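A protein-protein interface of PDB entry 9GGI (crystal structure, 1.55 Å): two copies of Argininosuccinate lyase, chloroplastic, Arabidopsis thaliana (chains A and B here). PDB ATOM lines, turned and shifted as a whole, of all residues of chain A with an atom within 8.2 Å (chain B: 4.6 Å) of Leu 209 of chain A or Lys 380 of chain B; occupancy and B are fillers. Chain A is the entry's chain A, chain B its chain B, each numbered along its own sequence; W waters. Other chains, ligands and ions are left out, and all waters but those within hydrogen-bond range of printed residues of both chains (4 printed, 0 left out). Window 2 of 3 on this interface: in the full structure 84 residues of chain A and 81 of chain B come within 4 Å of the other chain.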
ATOM      1  N   MET A  48     -23.966  20.057  -7.646  1.00  0.00           N
ATOM      2  CA  MET A  48     -25.137  20.012  -6.782  1.00  0.00           C
ATOM      3  C   MET A  48     -25.917  21.331  -6.845  1.00  0.00           C
ATOM      4  O   MET A  48     -27.138  21.319  -6.943  1.00  0.00           O
ATOM      5  CB  MET A  48     -24.759  19.610  -5.370  1.00  0.00           C
ATOM      6  CG  MET A  48     -25.883  19.613  -4.295  1.00  0.00           C
ATOM      7  SD  MET A  48     -26.246  21.276  -3.676  1.00  0.00           S
ATOM      8  CE  MET A  48     -24.749  21.589  -2.730  1.00  0.00           C
ATOM      9  N   LEU A  49     -25.247  22.447  -6.754  1.00  0.00           N
ATOM     10  CA  LEU A  49     -25.905  23.756  -6.847  1.00  0.00           C
ATOM     11  C   LEU A  49     -26.773  23.843  -8.107  1.00  0.00           C
ATOM     12  O   LEU A  49     -27.897  24.335  -8.027  1.00  0.00           O
ATOM     13  CB  LEU A  49     -24.898  24.892  -6.800  1.00  0.00           C
ATOM     14  CG  LEU A  49     -24.169  25.182  -5.495  1.00  0.00           C
ATOM     15  CD1 LEU A  49     -23.189  26.302  -5.697  1.00  0.00           C
ATOM     16  CD2 LEU A  49     -25.102  25.453  -4.319  1.00  0.00           C
ATOM     17  N   GLN A  52     -29.834  21.700  -7.945  1.00  0.00           N
ATOM     18  CA  GLN A  52     -30.802  22.235  -7.000  1.00  0.00           C
ATOM     19  C   GLN A  52     -31.361  23.587  -7.446  1.00  0.00           C
ATOM     20  O   GLN A  52     -32.122  24.171  -6.693  1.00  0.00           O
ATOM     21  CB  GLN A  52     -30.177  22.331  -5.610  1.00  0.00           C
ATOM     22  CG  GLN A  52     -29.818  20.961  -5.055  1.00  0.00           C
ATOM     23  CD  GLN A  52     -30.990  19.998  -5.013  1.00  0.00           C
ATOM     24  OE1 GLN A  52     -31.063  18.997  -5.737  1.00  0.00           O
ATOM     25  NE2 GLN A  52     -31.840  20.217  -4.019  1.00  0.00           N
ATOM     26  N   GLY A  53     -30.917  24.104  -8.577  1.00  0.00           N
ATOM     27  CA  GLY A  53     -31.436  25.336  -9.141  1.00  0.00           C
ATOM     28  C   GLY A  53     -30.891  26.589  -8.481  1.00  0.00           C
ATOM     29  O   GLY A  53     -31.410  27.688  -8.718  1.00  0.00           O
ATOM     30  N   LEU A  54     -29.776  26.460  -7.764  1.00  0.00           N
ATOM     31  CA  LEU A  54     -29.141  27.595  -7.101  1.00  0.00           C
ATOM     32  C   LEU A  54     -28.138  28.318  -7.986  1.00  0.00           C
ATOM     33  O   LEU A  54     -27.845  29.492  -7.705  1.00  0.00           O
ATOM     34  CB  LEU A  54     -28.444  27.146  -5.826  1.00  0.00           C
ATOM     35  CG  LEU A  54     -29.400  26.887  -4.668  1.00  0.00           C
ATOM     36  CD1 LEU A  54     -28.799  25.976  -3.594  1.00  0.00           C
ATOM     37  CD2 LEU A  54     -29.872  28.197  -4.080  1.00  0.00           C
ATOM     38  N   HIS A 108     -19.430  30.111  -3.892  1.00  0.00           N
ATOM     39  CA  HIS A 108     -19.482  30.309  -2.427  1.00  0.00           C
ATOM     40  C   HIS A 108     -20.903  30.066  -1.911  1.00  0.00           C
ATOM     41  O   HIS A 108     -21.105  30.059  -0.701  1.00  0.00           O
ATOM     42  CB  HIS A 108     -19.022  31.738  -2.110  1.00  0.00           C
ATOM     43  CG  HIS A 108     -18.608  32.026  -0.708  1.00  0.00           C
ATOM     44  ND1 HIS A 108     -19.169  31.455   0.411  1.00  0.00           N
ATOM     45  CD2 HIS A 108     -17.689  32.889  -0.258  1.00  0.00           C
ATOM     46  CE1 HIS A 108     -18.592  31.953   1.492  1.00  0.00           C
ATOM     47  NE2 HIS A 108     -17.691  32.826   1.109  1.00  0.00           N
ATOM     48  N   THR A 109     -21.887  30.029  -2.820  1.00  0.00           N
ATOM     49  CA  THR A 109     -23.276  29.840  -2.432  1.00  0.00           C
ATOM     50  C   THR A 109     -23.394  28.626  -1.544  1.00  0.00           C
ATOM     51  O   THR A 109     -22.989  27.532  -1.917  1.00  0.00           O
ATOM     52  CB  THR A 109     -24.141  29.711  -3.693  1.00  0.00           C
ATOM     53  OG1 THR A 109     -23.883  30.774  -4.600  1.00  0.00           O
ATOM     54  CG2 THR A 109     -25.613  29.657  -3.340  1.00  0.00           C
ATOM     55  N   ALA A 110     -24.027  28.805  -0.368  1.00  0.00           N
ATOM     56  CA  ALA A 110     -24.303  27.712   0.544  1.00  0.00           C
ATOM     57  C   ALA A 110     -23.047  26.937   0.875  1.00  0.00           C
ATOM     58  O   ALA A 110     -23.133  25.719   1.003  1.00  0.00           O
ATOM     59  CB  ALA A 110     -25.334  26.761  -0.014  1.00  0.00           C
ATOM     60  N   ARG A 111     -21.962  27.643   1.110  1.00  0.00           N
ATOM     61  CA  ARG A 111     -20.720  27.012   1.568  1.00  0.00           C
ATOM     62  C   ARG A 111     -19.876  28.029   2.300  1.00  0.00           C
ATOM     63  O   ARG A 111     -19.979  29.223   2.076  1.00  0.00           O
ATOM     64  CB  ARG A 111     -19.932  26.491   0.358  1.00  0.00           C
ATOM     65  CG  ARG A 111     -18.757  25.572   0.641  1.00  0.00           C
ATOM     66  CD  ARG A 111     -18.062  25.027  -0.575  1.00  0.00           C
ATOM     67  NE  ARG A 111     -17.355  26.135  -1.242  1.00  0.00           N
ATOM     68  CZ  ARG A 111     -16.547  26.031  -2.311  1.00  0.00           C
ATOM     69  NH1 ARG A 111     -16.263  24.873  -2.835  1.00  0.00           N
ATOM     70  NH2 ARG A 111     -15.968  27.107  -2.772  1.00  0.00           N
ATOM     71  N   GLY A 200     -21.777  21.052   3.461  1.00  0.00           N
ATOM     72  CA  GLY A 200     -23.164  21.472   3.632  1.00  0.00           C
ATOM     73  C   GLY A 200     -23.458  21.884   5.067  1.00  0.00           C
ATOM     74  O   GLY A 200     -24.547  22.338   5.394  1.00  0.00           O
ATOM     75  N   CYS A 202     -21.836  24.435   6.188  1.00  0.00           N
ATOM     76  CA  CYS A 202     -21.592  25.875   6.039  1.00  0.00           C
ATOM     77  C   CYS A 202     -20.748  26.353   7.209  1.00  0.00           C
ATOM     78  O   CYS A 202     -19.789  25.658   7.552  1.00  0.00           O
ATOM     79  CB  CYS A 202     -22.877  26.650   5.835  1.00  0.00           C
ATOM     80  SG  CYS A 202     -23.665  26.173   4.251  1.00  0.00           S
ATOM     81  N   GLY A 206     -25.408  24.875   9.224  1.00  0.00           N
ATOM     82  CA  GLY A 206     -26.110  24.520   7.994  1.00  0.00           C
ATOM     83  C   GLY A 206     -26.597  25.753   7.266  1.00  0.00           C
ATOM     84  O   GLY A 206     -26.069  26.863   7.441  1.00  0.00           O
ATOM     85  N   THR A 207     -27.652  25.546   6.470  1.00  0.00           N
ATOM     86  CA  THR A 207     -28.182  26.621   5.629  1.00  0.00           C
ATOM     87  C   THR A 207     -29.701  26.487   5.507  1.00  0.00           C
ATOM     88  O   THR A 207     -30.268  25.426   5.709  1.00  0.00           O
ATOM     89  CB  THR A 207     -27.485  26.574   4.257  1.00  0.00           C
ATOM     90  OG1 THR A 207     -27.987  27.629   3.413  1.00  0.00           O
ATOM     91  CG2 THR A 207     -27.631  25.260   3.538  1.00  0.00           C
ATOM     92  N   GLY A 208     -30.339  27.574   5.052  1.00  0.00           N
ATOM     93  CA  GLY A 208     -31.738  27.510   4.633  1.00  0.00           C
ATOM     94  C   GLY A 208     -31.892  27.371   3.124  1.00  0.00           C
ATOM     95  O   GLY A 208     -33.039  27.278   2.642  1.00  0.00           O
ATOM     96  N   LEU A 209     -30.783  27.323   2.391  1.00  0.00           N
ATOM     97  CA  LEU A 209     -30.805  27.188   0.939  1.00  0.00           C
ATOM     98  C   LEU A 209     -31.019  25.709   0.602  1.00  0.00           C
ATOM     99  O   LEU A 209     -30.593  24.842   1.382  1.00  0.00           O
ATOM    100  CB  LEU A 209     -29.545  27.723   0.299  1.00  0.00           C
ATOM    101  CG  LEU A 209     -29.333  29.230   0.452  1.00  0.00           C
ATOM    102  CD1 LEU A 209     -27.986  29.639  -0.042  1.00  0.00           C
ATOM    103  CD2 LEU A 209     -30.460  29.979  -0.288  1.00  0.00           C
ATOM    104  N   PRO A 210     -31.723  25.377  -0.510  1.00  0.00           N
ATOM    105  CA  PRO A 210     -32.112  24.001  -0.834  1.00  0.00           C
ATOM    106  C   PRO A 210     -30.990  23.132  -1.434  1.00  0.00           C
ATOM    107  O   PRO A 210     -31.084  22.606  -2.536  1.00  0.00           O
ATOM    108  CB  PRO A 210     -33.314  24.199  -1.787  1.00  0.00           C
ATOM    109  CG  PRO A 210     -32.973  25.468  -2.456  1.00  0.00           C
ATOM    110  CD  PRO A 210     -32.354  26.369  -1.406  1.00  0.00           C
ATOM    111  N   ILE A 211     -29.887  22.981  -0.671  1.00  0.00           N
ATOM    112  CA  ILE A 211     -28.816  22.089  -1.097  1.00  0.00           C
ATOM    113  C   ILE A 211     -29.237  20.633  -0.924  1.00  0.00           C
ATOM    114  O   ILE A 211     -30.279  20.303  -0.348  1.00  0.00           O
ATOM    115  CB  ILE A 211     -27.505  22.381  -0.342  1.00  0.00           C
ATOM    116  CG1 ILE A 211     -27.661  22.177   1.148  1.00  0.00           C
ATOM    117  CG2 ILE A 211     -27.014  23.798  -0.670  1.00  0.00           C
ATOM    118  CD1 ILE A 211     -26.381  22.242   1.966  1.00  0.00           C
ATOM    119  N   ASP A 212     -28.408  19.746  -1.450  1.00  0.00           N
ATOM    120  CA  ASP A 212     -28.587  18.319  -1.222  1.00  0.00           C
ATOM    121  C   ASP A 212     -27.237  17.735  -0.787  1.00  0.00           C
ATOM    122  O   ASP A 212     -26.357  17.488  -1.588  1.00  0.00           O
ATOM    123  CB  ASP A 212     -29.101  17.616  -2.466  1.00  0.00           C
ATOM    124  CG  ASP A 212     -29.364  16.135  -2.325  1.00  0.00           C
ATOM    125  OD1 ASP A 212     -28.958  15.577  -1.295  1.00  0.00           O
ATOM    126  OD2 ASP A 212     -30.055  15.605  -3.218  1.00  0.00           O
ATOM    127  N   ARG A 213     -27.124  17.487   0.504  1.00  0.00           N
ATOM    128  CA  ARG A 213     -25.874  16.988   1.066  1.00  0.00           C
ATOM    129  C   ARG A 213     -25.638  15.513   0.763  1.00  0.00           C
ATOM    130  O   ARG A 213     -24.490  15.090   0.761  1.00  0.00           O
ATOM    131  CB  ARG A 213     -25.876  17.197   2.583  1.00  0.00           C
ATOM    132  CG  ARG A 213     -25.840  18.656   2.998  1.00  0.00           C
ATOM    133  CD  ARG A 213     -25.682  18.893   4.502  1.00  0.00           C
ATOM    134  NE  ARG A 213     -24.407  18.342   4.964  1.00  0.00           N
ATOM    135  CZ  ARG A 213     -24.156  17.614   6.026  1.00  0.00           C
ATOM    136  NH1 ARG A 213     -25.092  17.382   6.914  1.00  0.00           N
ATOM    137  NH2 ARG A 213     -22.958  17.107   6.239  1.00  0.00           N
ATOM    138  N   ASP B 376     -29.610  34.492   2.621  1.00  0.00           N
ATOM    139  CA  ASP B 376     -30.293  33.336   2.038  1.00  0.00           C
ATOM    140  C   ASP B 376     -31.622  33.733   1.380  1.00  0.00           C
ATOM    141  O   ASP B 376     -31.983  33.219   0.315  1.00  0.00           O
ATOM    142  CB  ASP B 376     -30.558  32.227   3.044  1.00  0.00           C
ATOM    143  CG  ASP B 376     -29.359  31.430   3.555  1.00  0.00           C
ATOM    144  OD1 ASP B 376     -28.258  31.597   2.995  1.00  0.00           O
ATOM    145  OD2 ASP B 376     -29.567  30.570   4.493  1.00  0.00           O
ATOM    146  N   TYR B 377     -32.382  34.619   2.021  1.00  0.00           N
ATOM    147  CA  TYR B 377     -33.617  35.138   1.427  1.00  0.00           C
ATOM    148  C   TYR B 377     -33.322  35.688   0.034  1.00  0.00           C
ATOM    149  O   TYR B 377     -34.055  35.408  -0.932  1.00  0.00           O
ATOM    150  CB  TYR B 377     -34.202  36.209   2.343  1.00  0.00           C
ATOM    151  CG  TYR B 377     -35.345  37.022   1.739  1.00  0.00           C
ATOM    152  CD1 TYR B 377     -36.654  36.581   1.914  1.00  0.00           C
ATOM    153  CD2 TYR B 377     -35.132  38.252   1.183  1.00  0.00           C
ATOM    154  CE1 TYR B 377     -37.718  37.310   1.434  1.00  0.00           C
ATOM    155  CE2 TYR B 377     -36.185  38.986   0.669  1.00  0.00           C
ATOM    156  CZ  TYR B 377     -37.471  38.520   0.815  1.00  0.00           C
ATOM    157  OH  TYR B 377     -38.525  39.261   0.348  1.00  0.00           O
ATOM    158  N   LEU B 378     -32.322  36.550  -0.047  1.00  0.00           N
ATOM    159  CA  LEU B 378     -31.994  37.185  -1.321  1.00  0.00           C
ATOM    160  C   LEU B 378     -31.557  36.163  -2.379  1.00  0.00           C
ATOM    161  O   LEU B 378     -31.904  36.303  -3.562  1.00  0.00           O
ATOM    162  CB  LEU B 378     -30.953  38.244  -1.060  1.00  0.00           C
ATOM    163  CG  LEU B 378     -31.428  39.488  -0.289  1.00  0.00           C
ATOM    164  CD1 LEU B 378     -30.216  40.392   0.024  1.00  0.00           C
ATOM    165  CD2 LEU B 378     -32.470  40.290  -1.035  1.00  0.00           C
ATOM    166  N   VAL B 379     -30.728  35.171  -2.008  1.00  0.00           N
ATOM    167  CA  VAL B 379     -30.329  34.130  -2.945  1.00  0.00           C
ATOM    168  C   VAL B 379     -31.570  33.366  -3.407  1.00  0.00           C
ATOM    169  O   VAL B 379     -31.670  33.079  -4.597  1.00  0.00           O
ATOM    170  CB  VAL B 379     -29.242  33.206  -2.355  1.00  0.00           C
ATOM    171  CG1 VAL B 379     -28.984  31.961  -3.195  1.00  0.00           C
ATOM    172  CG2 VAL B 379     -27.943  33.970  -2.184  1.00  0.00           C
ATOM    173  N   LYS B 380     -32.500  33.080  -2.488  1.00  0.00           N
ATOM    174  CA  LYS B 380     -33.748  32.418  -2.832  1.00  0.00           C
ATOM    175  C   LYS B 380     -34.531  33.256  -3.837  1.00  0.00           C
ATOM    176  O   LYS B 380     -35.254  32.676  -4.631  1.00  0.00           O
ATOM    177  CB  LYS B 380     -34.602  32.103  -1.603  1.00  0.00           C
ATOM    178  CG  LYS B 380     -34.024  30.956  -0.806  1.00  0.00           C
ATOM    179  CD  LYS B 380     -34.589  30.842   0.619  1.00  0.00           C
ATOM    180  CE  LYS B 380     -34.388  29.518   1.224  1.00  0.00           C
ATOM    181  NZ  LYS B 380     -34.825  29.561   2.641  1.00  0.00           N
ATOM    182  N   LYS B 381     -34.539  34.577  -3.699  1.00  0.00           N
ATOM    183  CA  LYS B 381     -35.267  35.438  -4.622  1.00  0.00           C
ATOM    184  C   LYS B 381     -34.479  35.621  -5.921  1.00  0.00           C
ATOM    185  O   LYS B 381     -34.943  36.392  -6.747  1.00  0.00           O
ATOM    186  CB  LYS B 381     -35.501  36.829  -4.015  1.00  0.00           C
ATOM    187  CG  LYS B 381     -36.428  36.896  -2.785  1.00  0.00           C
ATOM    188  CD  LYS B 381     -37.853  36.523  -3.076  1.00  0.00           C
ATOM    189  CE  LYS B 381     -38.702  36.590  -1.832  1.00  0.00           C
ATOM    190  NZ  LYS B 381     -40.135  36.425  -2.107  1.00  0.00           N
ATOM    191  N   GLY B 382     -33.313  34.966  -6.127  1.00  0.00           N
ATOM    192  CA  GLY B 382     -32.576  35.008  -7.391  1.00  0.00           C
ATOM    193  C   GLY B 382     -31.357  35.923  -7.412  1.00  0.00           C
ATOM    194  O   GLY B 382     -30.757  36.181  -8.461  1.00  0.00           O
ATOM    195  N   PHE B 428     -38.174  36.196   7.772  1.00  0.00           N
ATOM    196  CA  PHE B 428     -36.806  35.721   7.694  1.00  0.00           C
ATOM    197  C   PHE B 428     -35.906  36.480   8.662  1.00  0.00           C
ATOM    198  O   PHE B 428     -34.677  36.284   8.636  1.00  0.00           O
ATOM    199  CB  PHE B 428     -36.217  35.900   6.306  1.00  0.00           C
ATOM    200  CG  PHE B 428     -36.882  34.979   5.296  1.00  0.00           C
ATOM    201  CD1 PHE B 428     -38.162  35.250   4.826  1.00  0.00           C
ATOM    202  CD2 PHE B 428     -36.219  33.853   4.824  1.00  0.00           C
ATOM    203  CE1 PHE B 428     -38.750  34.417   3.891  1.00  0.00           C
ATOM    204  CE2 PHE B 428     -36.800  33.022   3.893  1.00  0.00           C
ATOM    205  CZ  PHE B 428     -38.085  33.290   3.441  1.00  0.00           C
ATOM    206  N   SER B 439     -32.632  24.580   7.175  1.00  0.00           N
ATOM    207  CA  SER B 439     -33.416  23.472   6.656  1.00  0.00           C
ATOM    208  C   SER B 439     -32.560  22.319   6.131  1.00  0.00           C
ATOM    209  O   SER B 439     -33.123  21.295   5.771  1.00  0.00           O
ATOM    210  CB  SER B 439     -34.373  23.973   5.607  1.00  0.00           C
ATOM    211  OG  SER B 439     -33.656  24.560   4.528  1.00  0.00           O
HETATM  212  O   HOH W   1     -26.442  29.820   3.682  1.00  0.00           O
HETATM  213  O   HOH W   2     -35.273  27.780   4.623  1.00  0.00           O
HETATM  214  O   HOH W   3     -32.014  23.100   2.875  1.00  0.00           O
HETATM  215  O   HOH W   4     -34.701  25.365   1.304  1.00  0.00           O
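Gly 200 of chain A touches none of the printed residues of chain B. Printed residues of chain B within 4 Å of Thr 207 of chain A: Asp 376 and Ser 439. Printed residues of chain B within 4 Å of Gly 208 of chain A: Asp 376, Lys 380 and Ser 439. Leu 209 of chain A touches just these residues of chain B: Asp 376, Val 379 and Lys 380. Lys 380 of chain B touches just these residues of chain A: Gly 208 (2.9 Å) and Leu 209 (3.7 Å). Printed residues of chain A within 4 Å of Ser 439 of chain B: Thr 207 and Gly 208.
O of Leu 49 of chain A is in hydrogen-bond range of N of Leu 54 of chain A, 2.8 Å away. The side-chain hydroxyl (OG1) of Thr 207 of chain A is in hydrogen-bond range of the backbone NH (N) of Leu 209 of chain A (3.0 Å).
Of the 9 printed residues of chain B, 4 touch a printed residue of chain A. Printed residues of chain B that touch a printed residue of chain A: Asp 376, Val 379, Lys 380 and Ser 439. Of the 19 printed residues of chain A, 4 touch a printed residue of chain B. Hydrophobic or aromatic side chains of chain A that line the printed part of chain B: Leu 54 and Leu 209. Among the printed residues, 9 pairs touch across the chains. Among the printed residues, no Asp or Glu carboxylate lies within 4 Å of a Lys or Arg side-chain nitrogen of the other chain.
O of Thr 207 of chain A sits at hydrogen-bond distance from N of Ser 439 of chain B. The side-chain carboxylate (OD2) of Asp 376 of chain B is in hydrogen-bond range of the backbone NH (N) of Gly 208 of chain A, 3.1 Å away. The backbone carbonyl oxygen (O) of Gly 208 of chain A is in hydrogen-bond range of the side-chain amino group (NZ) of Lys 380 of chain B (2.9 Å). O of Gly 208 of chain A sits at hydrogen-bond distance from OG of Ser 439 of chain B, at 3.4 Å.
Among the printed residues, merely in contact across the chains: Leu 54 of chain A with Val 379 of chain B (3.97 Å), Thr 207 of chain A with Asp 376 of chain B (3.5 Å), Leu 209 of chain A with Asp 376 of chain B (3.6 Å), Leu 209 of chain A with Val 379 of chain B (3.8 Å) and Leu 209 of chain A with Lys 380 of chain B (3.7 Å).
No position is printed for both chains. Of the 9 pairs that touch across the chains among the printed residues, none has its exchanged pair printed and touching as well.
Water W1 bridges OD1 of Asp 376 of chain B and OG1 of Thr 207 of chain A. Water W3 bridges O of Leu 209 of chain A and OG of Ser 439 of chain B. Water W2 bridges the side-chain amino group of Lys 380 of chain B (2.7 Å) and the backbone carbonyl oxygen of Gly 208 of chain A (3.0 Å). Water W4 lies within hydrogen-bond range of O of Gly 208 of chain A (2.9 Å) and OG of Ser 439 of chain B (3.5 Å).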
